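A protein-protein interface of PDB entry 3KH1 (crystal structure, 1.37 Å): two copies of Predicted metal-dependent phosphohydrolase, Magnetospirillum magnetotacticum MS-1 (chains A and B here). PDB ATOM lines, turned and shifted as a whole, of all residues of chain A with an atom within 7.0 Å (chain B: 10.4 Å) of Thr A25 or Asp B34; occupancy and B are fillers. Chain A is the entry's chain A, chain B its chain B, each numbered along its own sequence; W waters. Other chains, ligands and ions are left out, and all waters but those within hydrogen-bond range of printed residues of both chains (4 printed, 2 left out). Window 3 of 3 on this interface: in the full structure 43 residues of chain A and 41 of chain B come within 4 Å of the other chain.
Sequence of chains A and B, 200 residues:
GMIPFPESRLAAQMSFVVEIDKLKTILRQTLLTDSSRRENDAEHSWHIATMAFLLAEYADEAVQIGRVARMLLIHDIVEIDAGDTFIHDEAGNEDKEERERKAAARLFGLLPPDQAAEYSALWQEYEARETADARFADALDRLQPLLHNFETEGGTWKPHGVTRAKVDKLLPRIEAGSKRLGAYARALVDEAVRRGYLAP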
ATOM      1  N   ILE A  20     -21.516   2.565 -16.789  1.00  0.00           N
ATOM      2  CA  ILE A  20     -21.321   3.508 -17.887  1.00  0.00           C
ATOM      3  C   ILE A  20     -21.275   2.830 -19.241  1.00  0.00           C
ATOM      4  O   ILE A  20     -21.264   3.544 -20.250  1.00  0.00           O
ATOM      5  CB  ILE A  20     -20.127   4.478 -17.628  1.00  0.00           C
ATOM      6  CG1 ILE A  20     -18.780   3.764 -17.636  1.00  0.00           C
ATOM      7  CG2 ILE A  20     -20.342   5.316 -16.361  1.00  0.00           C
ATOM      8  CD1 ILE A  20     -17.536   4.717 -17.537  1.00  0.00           C
ATOM      9  N   ASP A  21     -21.286   1.490 -19.324  1.00  0.00           N
ATOM     10  CA  ASP A  21     -21.624   0.831 -20.587  1.00  0.00           C
ATOM     11  C   ASP A  21     -22.829   1.467 -21.246  1.00  0.00           C
ATOM     12  O   ASP A  21     -22.944   1.488 -22.495  1.00  0.00           O
ATOM     13  CB  ASP A  21     -21.884  -0.686 -20.415  1.00  0.00           C
ATOM     14  CG  ASP A  21     -21.855  -1.476 -21.763  1.00  0.00           C
ATOM     15  OD1 ASP A  21     -20.743  -1.675 -22.270  1.00  0.00           O
ATOM     16  OD2 ASP A  21     -22.922  -1.973 -22.249  1.00  0.00           O
ATOM     17  N   LYS A  22     -23.777   1.916 -20.414  1.00  0.00           N
ATOM     18  CA  LYS A  22     -25.038   2.440 -20.917  1.00  0.00           C
ATOM     19  C   LYS A  22     -24.887   3.689 -21.770  1.00  0.00           C
ATOM     20  O   LYS A  22     -25.791   4.025 -22.538  1.00  0.00           O
ATOM     21  CB  LYS A  22     -25.962   2.713 -19.749  1.00  0.00           C
ATOM     22  CG  LYS A  22     -26.386   1.455 -19.002  1.00  0.00           C
ATOM     23  CD  LYS A  22     -27.286   1.832 -17.793  1.00  0.00           C
ATOM     24  CE  LYS A  22     -27.734   0.655 -16.959  1.00  0.00           C
ATOM     25  NZ  LYS A  22     -28.575   1.149 -15.785  1.00  0.00           N
ATOM     26  N   LEU A  23     -23.753   4.374 -21.695  1.00  0.00           N
ATOM     27  CA  LEU A  23     -23.564   5.577 -22.533  1.00  0.00           C
ATOM     28  C   LEU A  23     -23.601   5.215 -24.011  1.00  0.00           C
ATOM     29  O   LEU A  23     -23.923   6.032 -24.878  1.00  0.00           O
ATOM     30  CB  LEU A  23     -22.270   6.294 -22.155  1.00  0.00           C
ATOM     31  CG  LEU A  23     -22.064   7.651 -22.833  1.00  0.00           C
ATOM     32  CD1 LEU A  23     -23.180   8.609 -22.383  1.00  0.00           C
ATOM     33  CD2 LEU A  23     -20.701   8.166 -22.520  1.00  0.00           C
ATOM     34  N   LYS A  24     -23.238   3.976 -24.307  1.00  0.00           N
ATOM     35  CA  LYS A  24     -23.177   3.464 -25.677  1.00  0.00           C
ATOM     36  C   LYS A  24     -24.543   3.438 -26.354  1.00  0.00           C
ATOM     37  O   LYS A  24     -24.574   3.425 -27.588  1.00  0.00           O
ATOM     38  CB  LYS A  24     -22.555   2.055 -25.664  1.00  0.00           C
ATOM     39  CG  LYS A  24     -21.079   2.066 -25.179  1.00  0.00           C
ATOM     40  CD  LYS A  24     -20.555   0.680 -24.851  1.00  0.00           C
ATOM     41  CE  LYS A  24     -19.202   0.742 -24.160  1.00  0.00           C
ATOM     42  NZ  LYS A  24     -18.725  -0.626 -23.719  1.00  0.00           N
ATOM     43  N   THR A  25     -25.610   3.498 -25.581  1.00  0.00           N
ATOM     44  CA  THR A  25     -26.965   3.411 -26.069  1.00  0.00           C
ATOM     45  C   THR A  25     -27.616   4.781 -26.281  1.00  0.00           C
ATOM     46  O   THR A  25     -28.748   4.848 -26.726  1.00  0.00           O
ATOM     47  CB  THR A  25     -27.895   2.576 -25.052  1.00  0.00           C
ATOM     48  OG1 THR A  25     -28.098   3.332 -23.866  1.00  0.00           O
ATOM     49  CG2 THR A  25     -27.302   1.311 -24.677  1.00  0.00           C
ATOM     50  N   ILE A  26     -26.915   5.866 -25.952  1.00  0.00           N
ATOM     51  CA  ILE A  26     -27.468   7.237 -26.061  1.00  0.00           C
ATOM     52  C   ILE A  26     -27.068   7.796 -27.410  1.00  0.00           C
ATOM     53  O   ILE A  26     -25.866   7.951 -27.728  1.00  0.00           O
ATOM     54  CB  ILE A  26     -26.987   8.142 -24.939  1.00  0.00           C
ATOM     55  CG1 ILE A  26     -27.266   7.548 -23.556  1.00  0.00           C
ATOM     56  CG2 ILE A  26     -27.619   9.560 -25.074  1.00  0.00           C
ATOM     57  CD1 ILE A  26     -28.746   7.295 -23.260  1.00  0.00           C
ATOM     58  N   LEU A  27     -28.048   8.086 -28.238  1.00  0.00           N
ATOM     59  CA  LEU A  27     -27.814   8.516 -29.637  1.00  0.00           C
ATOM     60  C   LEU A  27     -27.926  10.022 -29.854  1.00  0.00           C
ATOM     61  O   LEU A  27     -28.796  10.701 -29.308  1.00  0.00           O
ATOM     62  CB  LEU A  27     -28.786   7.811 -30.577  1.00  0.00           C
ATOM     63  CG  LEU A  27     -28.671   6.272 -30.485  1.00  0.00           C
ATOM     64  CD1 LEU A  27     -29.608   5.538 -31.371  1.00  0.00           C
ATOM     65  CD2 LEU A  27     -27.194   5.803 -30.702  1.00  0.00           C
ATOM     66  N   ASN A  40     -23.310   7.463 -31.420  1.00  0.00           N
ATOM     67  CA  ASN A  40     -23.646   7.370 -30.031  1.00  0.00           C
ATOM     68  C   ASN A  40     -22.708   8.201 -29.146  1.00  0.00           C
ATOM     69  O   ASN A  40     -21.624   8.623 -29.561  1.00  0.00           O
ATOM     70  CB  ASN A  40     -23.827   5.907 -29.563  1.00  0.00           C
ATOM     71  CG  ASN A  40     -22.527   5.172 -29.354  1.00  0.00           C
ATOM     72  OD1 ASN A  40     -21.666   5.586 -28.541  1.00  0.00           O
ATOM     73  ND2 ASN A  40     -22.379   4.015 -30.016  1.00  0.00           N
ATOM     74  N   ASP A  41     -23.106   8.448 -27.897  1.00  0.00           N
ATOM     75  CA  ASP A  41     -22.334   9.315 -27.027  1.00  0.00           C
ATOM     76  C   ASP A  41     -20.963   8.735 -26.696  1.00  0.00           C
ATOM     77  O   ASP A  41     -20.020   9.497 -26.500  1.00  0.00           O
ATOM     78  CB  ASP A  41     -23.072   9.589 -25.706  1.00  0.00           C
ATOM     79  CG  ASP A  41     -24.047  10.715 -25.780  1.00  0.00           C
ATOM     80  OD1 ASP A  41     -24.255  11.320 -26.849  1.00  0.00           O
ATOM     81  OD2 ASP A  41     -24.604  11.004 -24.687  1.00  0.00           O
ATOM     82  N   ALA A  42     -20.858   7.419 -26.517  1.00  0.00           N
ATOM     83  CA  ALA A  42     -19.562   6.813 -26.146  1.00  0.00           C
ATOM     84  C   ALA A  42     -18.586   6.969 -27.298  1.00  0.00           C
ATOM     85  O   ALA A  42     -17.445   7.377 -27.096  1.00  0.00           O
ATOM     86  CB  ALA A  42     -19.738   5.331 -25.759  1.00  0.00           C
ATOM     87  N   ILE A  80     -26.672   9.300 -19.835  1.00  0.00           N
ATOM     88  CA  ILE A  80     -27.227   7.973 -19.536  1.00  0.00           C
ATOM     89  C   ILE A  80     -28.633   8.102 -19.006  1.00  0.00           C
ATOM     90  O   ILE A  80     -29.494   7.307 -19.382  1.00  0.00           O
ATOM     91  CB  ILE A  80     -26.319   7.165 -18.588  1.00  0.00           C
ATOM     92  CG1 ILE A  80     -25.031   6.751 -19.293  1.00  0.00           C
ATOM     93  CG2 ILE A  80     -27.049   5.965 -17.993  1.00  0.00           C
ATOM     94  CD1 ILE A  80     -23.937   6.333 -18.368  1.00  0.00           C
ATOM     95  N   THR B  30     -18.516  -9.178 -28.737  1.00  0.00           N
ATOM     96  CA  THR B  30     -19.218  -8.771 -27.507  1.00  0.00           C
ATOM     97  C   THR B  30     -20.533  -8.107 -27.821  1.00  0.00           C
ATOM     98  O   THR B  30     -20.552  -7.214 -28.669  1.00  0.00           O
ATOM     99  CB  THR B  30     -18.350  -7.687 -26.773  1.00  0.00           C
ATOM    100  OG1 THR B  30     -17.065  -8.216 -26.485  1.00  0.00           O
ATOM    101  CG2 THR B  30     -18.990  -7.154 -25.496  1.00  0.00           C
ATOM    102  N   LEU B  31     -21.592  -8.464 -27.117  1.00  0.00           N
ATOM    103  CA  LEU B  31     -22.776  -7.645 -27.125  1.00  0.00           C
ATOM    104  C   LEU B  31     -22.637  -6.598 -25.999  1.00  0.00           C
ATOM    105  O   LEU B  31     -21.801  -6.754 -25.037  1.00  0.00           O
ATOM    106  CB  LEU B  31     -23.981  -8.505 -26.983  1.00  0.00           C
ATOM    107  CG  LEU B  31     -24.249  -9.565 -28.055  1.00  0.00           C
ATOM    108  CD1 LEU B  31     -25.440 -10.429 -27.626  1.00  0.00           C
ATOM    109  CD2 LEU B  31     -24.455  -8.989 -29.451  1.00  0.00           C
ATOM    110  N   LEU B  32     -23.438  -5.548 -26.099  1.00  0.00           N
ATOM    111  CA  LEU B  32     -23.576  -4.605 -25.003  1.00  0.00           C
ATOM    112  C   LEU B  32     -24.147  -5.260 -23.791  1.00  0.00           C
ATOM    113  O   LEU B  32     -24.651  -6.360 -23.872  1.00  0.00           O
ATOM    114  CB  LEU B  32     -24.405  -3.408 -25.409  1.00  0.00           C
ATOM    115  CG  LEU B  32     -23.947  -2.496 -26.544  1.00  0.00           C
ATOM    116  CD1 LEU B  32     -24.941  -1.336 -26.594  1.00  0.00           C
ATOM    117  CD2 LEU B  32     -22.557  -2.068 -26.434  1.00  0.00           C
ATOM    118  N   THR B  33     -23.972  -4.628 -22.614  1.00  0.00           N
ATOM    119  CA  THR B  33     -24.486  -5.228 -21.363  1.00  0.00           C
ATOM    120  C   THR B  33     -25.985  -5.428 -21.389  1.00  0.00           C
ATOM    121  O   THR B  33     -26.501  -6.329 -20.755  1.00  0.00           O
ATOM    122  CB  THR B  33     -24.099  -4.412 -20.085  1.00  0.00           C
ATOM    123  OG1 THR B  33     -24.765  -3.144 -20.102  1.00  0.00           O
ATOM    124  CG2 THR B  33     -22.593  -4.210 -20.030  1.00  0.00           C
ATOM    125  N   ASP B  34     -26.708  -4.632 -22.168  1.00  0.00           N
ATOM    126  CA  ASP B  34     -28.120  -4.864 -22.406  1.00  0.00           C
ATOM    127  C   ASP B  34     -28.477  -5.856 -23.517  1.00  0.00           C
ATOM    128  O   ASP B  34     -29.663  -6.065 -23.824  1.00  0.00           O
ATOM    129  CB  ASP B  34     -28.872  -3.521 -22.567  1.00  0.00           C
ATOM    130  CG  ASP B  34     -28.601  -2.830 -23.882  1.00  0.00           C
ATOM    131  OD1 ASP B  34     -27.819  -3.347 -24.696  1.00  0.00           O
ATOM    132  OD2 ASP B  34     -29.226  -1.778 -24.104  1.00  0.00           O
ATOM    133  N   SER B  35     -27.450  -6.508 -24.073  1.00  0.00           N
ATOM    134  CA  SER B  35     -27.587  -7.479 -25.189  1.00  0.00           C
ATOM    135  C   SER B  35     -28.253  -6.941 -26.448  1.00  0.00           C
ATOM    136  O   SER B  35     -28.651  -7.706 -27.324  1.00  0.00           O
ATOM    137  CB  SER B  35     -28.298  -8.757 -24.739  1.00  0.00           C
ATOM    138  OG  SER B  35     -27.674  -9.393 -23.621  1.00  0.00           O
ATOM    139  N   SER B  36     -28.346  -5.621 -26.594  1.00  0.00           N
ATOM    140  CA  SER B  36     -29.072  -5.041 -27.718  1.00  0.00           C
ATOM    141  C   SER B  36     -28.364  -5.120 -29.075  1.00  0.00           C
ATOM    142  O   SER B  36     -29.013  -5.143 -30.089  1.00  0.00           O
ATOM    143  CB  SER B  36     -29.428  -3.598 -27.410  1.00  0.00           C
ATOM    144  OG  SER B  36     -28.298  -2.753 -27.243  1.00  0.00           O
ATOM    145  N   ARG B  37     -27.045  -5.097 -29.061  1.00  0.00           N
ATOM    146  CA  ARG B  37     -26.240  -5.044 -30.282  1.00  0.00           C
ATOM    147  C   ARG B  37     -24.806  -5.354 -29.910  1.00  0.00           C
ATOM    148  O   ARG B  37     -24.401  -5.333 -28.741  1.00  0.00           O
ATOM    149  CB  ARG B  37     -26.347  -3.653 -30.938  1.00  0.00           C
ATOM    150  CG  ARG B  37     -25.782  -2.533 -30.108  1.00  0.00           C
ATOM    151  CD  ARG B  37     -25.780  -1.219 -30.942  1.00  0.00           C
ATOM    152  NE  ARG B  37     -25.298  -0.088 -30.171  1.00  0.00           N
ATOM    153  CZ  ARG B  37     -24.024   0.134 -29.870  1.00  0.00           C
ATOM    154  NH1 ARG B  37     -23.056  -0.692 -30.274  1.00  0.00           N
ATOM    155  NH2 ARG B  37     -23.691   1.190 -29.129  1.00  0.00           N
ATOM    156  N   ARG B  38     -24.025  -5.591 -30.952  1.00  0.00           N
ATOM    157  CA  ARG B  38     -22.580  -5.771 -30.844  1.00  0.00           C
ATOM    158  C   ARG B  38     -21.880  -4.492 -30.458  1.00  0.00           C
ATOM    159  O   ARG B  38     -22.159  -3.427 -30.988  1.00  0.00           O
ATOM    160  CB  ARG B  38     -22.044  -6.277 -32.176  1.00  0.00           C
ATOM    161  CG  ARG B  38     -22.542  -7.667 -32.521  1.00  0.00           C
ATOM    162  CD  ARG B  38     -22.222  -8.074 -33.929  1.00  0.00           C
ATOM    163  NE  ARG B  38     -20.786  -8.283 -34.122  1.00  0.00           N
ATOM    164  CZ  ARG B  38     -20.247  -8.617 -35.290  1.00  0.00           C
ATOM    165  NH1 ARG B  38     -20.981  -8.833 -36.359  1.00  0.00           N
ATOM    166  NH2 ARG B  38     -18.934  -8.700 -35.393  1.00  0.00           N
ATOM    167  N   GLU B  39     -20.895  -4.581 -29.569  1.00  0.00           N
ATOM    168  CA  GLU B  39     -20.009  -3.496 -29.266  1.00  0.00           C
ATOM    169  C   GLU B  39     -19.078  -3.184 -30.427  1.00  0.00           C
ATOM    170  O   GLU B  39     -18.619  -4.093 -31.086  1.00  0.00           O
ATOM    171  CB  GLU B  39     -19.218  -3.793 -28.002  1.00  0.00           C
ATOM    172  CG  GLU B  39     -18.426  -2.646 -27.433  1.00  0.00           C
ATOM    173  CD  GLU B  39     -17.498  -3.012 -26.291  1.00  0.00           C
ATOM    174  OE1 GLU B  39     -17.003  -4.162 -26.288  1.00  0.00           O
ATOM    175  OE2 GLU B  39     -17.162  -2.141 -25.475  1.00  0.00           O
ATOM    176  N   ASN B  40     -18.795  -1.897 -30.657  1.00  0.00           N
ATOM    177  CA  ASN B  40     -17.808  -1.519 -31.655  1.00  0.00           C
ATOM    178  C   ASN B  40     -16.480  -1.084 -31.037  1.00  0.00           C
ATOM    179  O   ASN B  40     -16.359  -0.831 -29.840  1.00  0.00           O
ATOM    180  CB  ASN B  40     -18.335  -0.500 -32.671  1.00  0.00           C
ATOM    181  CG  ASN B  40     -18.498   0.911 -32.129  1.00  0.00           C
ATOM    182  OD1 ASN B  40     -17.496   1.524 -31.704  1.00  0.00           O
ATOM    183  ND2 ASN B  40     -19.723   1.435 -32.103  1.00  0.00           N
ATOM    184  N   GLU B  43     -16.315   2.715 -29.268  1.00  0.00           N
ATOM    185  CA  GLU B  43     -16.914   2.850 -27.967  1.00  0.00           C
ATOM    186  C   GLU B  43     -16.181   1.960 -26.948  1.00  0.00           C
ATOM    187  O   GLU B  43     -16.107   2.291 -25.759  1.00  0.00           O
ATOM    188  CB  GLU B  43     -18.391   2.563 -28.021  1.00  0.00           C
ATOM    189  CG  GLU B  43     -18.746   1.128 -28.373  1.00  0.00           C
ATOM    190  CD  GLU B  43     -20.181   0.909 -28.792  1.00  0.00           C
ATOM    191  OE1 GLU B  43     -20.977   1.862 -28.739  1.00  0.00           O
ATOM    192  OE2 GLU B  43     -20.505  -0.228 -29.154  1.00  0.00           O
ATOM    193  N   TRP B  46     -13.230   4.091 -25.892  1.00  0.00           N
ATOM    194  CA  TRP B  46     -13.719   5.073 -24.964  1.00  0.00           C
ATOM    195  C   TRP B  46     -13.783   4.467 -23.528  1.00  0.00           C
ATOM    196  O   TRP B  46     -13.316   5.055 -22.545  1.00  0.00           O
ATOM    197  CB  TRP B  46     -15.171   5.514 -25.314  1.00  0.00           C
ATOM    198  CG  TRP B  46     -15.850   6.227 -24.182  1.00  0.00           C
ATOM    199  CD1 TRP B  46     -15.647   7.513 -23.765  1.00  0.00           C
ATOM    200  CD2 TRP B  46     -16.789   5.653 -23.250  1.00  0.00           C
ATOM    201  NE1 TRP B  46     -16.388   7.766 -22.633  1.00  0.00           N
ATOM    202  CE2 TRP B  46     -17.066   6.635 -22.297  1.00  0.00           C
ATOM    203  CE3 TRP B  46     -17.408   4.381 -23.126  1.00  0.00           C
ATOM    204  CZ2 TRP B  46     -17.962   6.428 -21.251  1.00  0.00           C
ATOM    205  CZ3 TRP B  46     -18.282   4.181 -22.079  1.00  0.00           C
ATOM    206  CH2 TRP B  46     -18.551   5.200 -21.178  1.00  0.00           C
ATOM    207  N   HIS B  47     -14.324   3.257 -23.441  1.00  0.00           N
ATOM    208  CA  HIS B  47     -14.596   2.665 -22.140  1.00  0.00           C
ATOM    209  C   HIS B  47     -13.274   2.386 -21.422  1.00  0.00           C
ATOM    210  O   HIS B  47     -13.128   2.658 -20.231  1.00  0.00           O
ATOM    211  CB  HIS B  47     -15.397   1.361 -22.324  1.00  0.00           C
ATOM    212  CG  HIS B  47     -16.218   0.937 -21.145  1.00  0.00           C
ATOM    213  ND1 HIS B  47     -17.246   0.028 -21.287  1.00  0.00           N
ATOM    214  CD2 HIS B  47     -16.234   1.328 -19.850  1.00  0.00           C
ATOM    215  CE1 HIS B  47     -17.828  -0.140 -20.111  1.00  0.00           C
ATOM    216  NE2 HIS B  47     -17.220   0.608 -19.217  1.00  0.00           N
ATOM    217  N   GLN B 144     -11.691  -5.414 -18.663  1.00  0.00           N
ATOM    218  CA  GLN B 144     -13.028  -4.963 -18.976  1.00  0.00           C
ATOM    219  C   GLN B 144     -13.964  -6.103 -19.426  1.00  0.00           C
ATOM    220  O   GLN B 144     -15.098  -6.167 -18.935  1.00  0.00           O
ATOM    221  CB  GLN B 144     -12.977  -3.793 -19.972  1.00  0.00           C
ATOM    222  CG  GLN B 144     -14.356  -3.137 -20.202  1.00  0.00           C
ATOM    223  CD  GLN B 144     -15.188  -3.873 -21.157  1.00  0.00           C
ATOM    224  OE1 GLN B 144     -14.653  -4.592 -22.013  1.00  0.00           O
ATOM    225  NE2 GLN B 144     -16.524  -3.715 -21.032  1.00  0.00           N
ATOM    226  N   HIS B 148     -17.640  -7.202 -17.845  1.00  0.00           N
ATOM    227  CA  HIS B 148     -18.798  -7.334 -18.710  1.00  0.00           C
ATOM    228  C   HIS B 148     -19.430  -8.705 -18.618  1.00  0.00           C
ATOM    229  O   HIS B 148     -20.661  -8.834 -18.441  1.00  0.00           O
ATOM    230  CB  HIS B 148     -18.451  -6.987 -20.157  1.00  0.00           C
ATOM    231  CG  HIS B 148     -19.541  -7.320 -21.115  1.00  0.00           C
ATOM    232  ND1 HIS B 148     -20.594  -6.468 -21.350  1.00  0.00           N
ATOM    233  CD2 HIS B 148     -19.789  -8.439 -21.843  1.00  0.00           C
ATOM    234  CE1 HIS B 148     -21.436  -7.037 -22.189  1.00  0.00           C
ATOM    235  NE2 HIS B 148     -20.984  -8.239 -22.500  1.00  0.00           N
ATOM    236  N   ASN B 149     -18.602  -9.742 -18.759  1.00  0.00           N
ATOM    237  CA  ASN B 149     -19.082 -11.105 -18.697  1.00  0.00           C
ATOM    238  C   ASN B 149     -19.700 -11.418 -17.328  1.00  0.00           C
ATOM    239  O   ASN B 149     -20.725 -12.094 -17.266  1.00  0.00           O
ATOM    240  CB  ASN B 149     -17.989 -12.112 -19.015  1.00  0.00           C
ATOM    241  CG  ASN B 149     -17.877 -12.423 -20.497  1.00  0.00           C
ATOM    242  OD1 ASN B 149     -18.767 -13.068 -21.075  1.00  0.00           O
ATOM    243  ND2 ASN B 149     -16.780 -12.040 -21.100  1.00  0.00           N
ATOM    244  N   GLU B 151     -21.154  -9.273 -15.319  1.00  0.00           N
ATOM    245  CA  GLU B 151     -22.416  -8.528 -15.294  1.00  0.00           C
ATOM    246  C   GLU B 151     -23.525  -9.191 -16.131  1.00  0.00           C
ATOM    247  O   GLU B 151     -24.692  -9.142 -15.755  1.00  0.00           O
ATOM    248  CB  GLU B 151     -22.170  -7.079 -15.756  1.00  0.00           C
ATOM    249  CG  GLU B 151     -23.416  -6.204 -15.890  1.00  0.00           C
ATOM    250  CD  GLU B 151     -24.136  -5.875 -14.581  1.00  0.00           C
ATOM    251  OE1 GLU B 151     -23.583  -6.067 -13.471  1.00  0.00           O
ATOM    252  OE2 GLU B 151     -25.306  -5.400 -14.690  1.00  0.00           O
ATOM    253  N   THR B 152     -23.160  -9.794 -17.262  1.00  0.00           N
ATOM    254  CA  THR B 152     -24.115 -10.444 -18.168  1.00  0.00           C
ATOM    255  C   THR B 152     -24.198 -11.974 -17.985  1.00  0.00           C
ATOM    256  O   THR B 152     -24.776 -12.651 -18.827  1.00  0.00           O
ATOM    257  CB  THR B 152     -23.750 -10.165 -19.601  1.00  0.00           C
ATOM    258  OG1 THR B 152     -22.451 -10.693 -19.863  1.00  0.00           O
ATOM    259  CG2 THR B 152     -23.746  -8.660 -19.879  1.00  0.00           C
ATOM    260  N   GLU B 153     -23.644 -12.491 -16.896  1.00  0.00           N
ATOM    261  CA  GLU B 153     -23.748 -13.913 -16.571  1.00  0.00           C
ATOM    262  C   GLU B 153     -23.118 -14.791 -17.699  1.00  0.00           C
ATOM    263  O   GLU B 153     -23.666 -15.835 -18.077  1.00  0.00           O
ATOM    264  CB  GLU B 153     -25.229 -14.274 -16.272  1.00  0.00           C
ATOM    265  CG  GLU B 153     -25.822 -13.672 -14.952  1.00  0.00           C
ATOM    266  CD  GLU B 153     -26.319 -12.204 -15.020  1.00  0.00           C
ATOM    267  OE1 GLU B 153     -26.770 -11.733 -16.080  1.00  0.00           O
ATOM    268  OE2 GLU B 153     -26.281 -11.516 -13.976  1.00  0.00           O
ATOM    269  N   GLY B 155     -22.209 -13.533 -20.897  1.00  0.00           N
ATOM    270  CA  GLY B 155     -22.860 -13.222 -22.186  1.00  0.00           C
ATOM    271  C   GLY B 155     -21.969 -13.363 -23.418  1.00  0.00           C
ATOM    272  O   GLY B 155     -22.492 -13.568 -24.532  1.00  0.00           O
ATOM    273  N   THR B 156     -20.656 -13.235 -23.241  1.00  0.00           N
ATOM    274  CA  THR B 156     -19.707 -13.432 -24.355  1.00  0.00           C
ATOM    275  C   THR B 156     -19.068 -14.822 -24.277  1.00  0.00           C
ATOM    276  O   THR B 156     -18.933 -15.528 -25.273  1.00  0.00           O
ATOM    277  CB  THR B 156     -18.622 -12.345 -24.431  1.00  0.00           C
ATOM    278  OG1 THR B 156     -19.192 -11.051 -24.155  1.00  0.00           O
ATOM    279  CG2 THR B 156     -17.933 -12.328 -25.814  1.00  0.00           C
HETATM  280  O   HOH W   1     -25.615  -1.544 -22.225  1.00  0.00           O
HETATM  281  O   HOH W   2     -26.998   2.203 -29.675  1.00  0.00           O
HETATM  282  O   HOH W   3     -20.307  -3.867 -24.191  1.00  0.00           O
HETATM  283  O   HOH W   4     -16.006  -1.899 -23.263  1.00  0.00           O
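Hydrophobic or aromatic side chains of chain B within 4 Å of the printed part of chain A: Leu B32, Trp B46 and His B47. Printed residues of chain A that touch a printed residue of chain B: Ile A20, Asp A21, Leu A23, Lys A24, Thr A25, Asn A40 and Ala A42. Hydrophobic or aromatic side chains of chain A that line the printed part of chain B: Ile A20, Leu A23 and Ala A42. Among the printed residues, Asp or Glu carboxylates within 4 Å of a Lys or Arg side-chain nitrogen of the other chain: Lys A24 with Glu B39.
Thr A25 touches just one residue of chain B: Asp B34. Of chain A, only Thr A25 (3.7 Å) comes within 4 Å of Asp B34. Printed residues of chain A within 4 Å of Glu B39: Lys A24 (2.8 Å). Of the printed residues of chain B, Ile A20 touches Trp B46 and His B47. The nearest residue of chain B that does not touch Thr A25 is Leu B32 (4.03 Å). The nearest printed residue of chain A that does not touch His B47 is Ala A42 (6.2 Å).
The backbone carbonyl oxygen (O) of Lys A24 lies close to the side-chain amide nitrogen (ND2) of Asn A40. The side-chain carboxylate (OD1) of Asp A21 lies within salt-bridge range of the side-chain amino group (NZ) of Lys A24 (2.7 Å). The backbone NH of Ala A42 sits at hydrogen-bond distance from the side-chain amide oxygen of Asn A40, 2.8 Å away. OE1 of Glu B43 lies within salt-bridge range of NH2 of Arg B37, 2.8 Å away. O of Lys A22 is in hydrogen-bond range of OG1 of Thr A25 (2.8 Å). The backbone NH (N) of Leu B32 lies within hydrogen-bond range of the backbone carbonyl oxygen (O) of Arg B37 (2.8 Å).
Water W4 lies within hydrogen-bond range of the side-chain carboxylate of Glu B39, the side-chain amide nitrogen of Gln B144, a ring nitrogen (ND1) of His B47 and the side-chain amino group of Lys A24. Water W1 lies within hydrogen-bond range of OD2 of Asp A21 (2.7 Å), OG1 of Thr B33 (2.8 Å) and N of Asp B34 (3.3 Å). Water W2 lies within hydrogen-bond range of the guanidinium group (NE) of Arg B37 and the backbone carbonyl oxygen (O) of Lys A24. Water W3 bridges OD1 of Asp A21 and O of Leu B31.
Ile A20 touches Trp B46 (O to CH2, 3.3 Å). NE2 of His B47 touches CG1 of Ile A20 (3.9 Å). Asp A21 touches Leu B32. Asp A21 touches His B47. CZ2 of Trp B46 touches CD2 of Leu A23, 3.5 Å away. Lys A24 touches Leu B32. OE1 of Glu B43 touches CB of Lys A24, at 3.5 Å. Thr A25 touches Asp B34 (CG2 to OD2, 3.7 Å). CB of Ala A42 touches CB of Glu B43 (3.8 Å). O of Ala A42 touches CB of Trp B46, at 3.4 Å.
The side-chain amide nitrogen (ND2) of Asn A40 lies within hydrogen-bond range of the side-chain carboxylate (OE1) of Glu B43, at 2.9 Å. The side-chain amino group of Lys A24 sits at hydrogen-bond distance from a ring nitrogen (ND1) of His B47, at 2.9 Å. The side-chain amide nitrogen of Asn A40 lies close to the guanidinium group of Arg B37, at 3.2 Å. The backbone carbonyl oxygen (O) of Lys A24 sits at hydrogen-bond distance from the guanidinium group (NH2) of Arg B37 (2.9 Å). The backbone NH (N) of Thr B33 sits at hydrogen-bond distance from the side-chain carboxylate (OD2) of Asp A21, 2.9 Å away. The side-chain carboxylate of Glu B39 is in salt-bridge range of the side-chain amino group of Lys A24.
1 position is printed for both chains. Of the 16 pairs that touch across the chains among the printed residues, none has its exchanged pair printed and touching as well.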
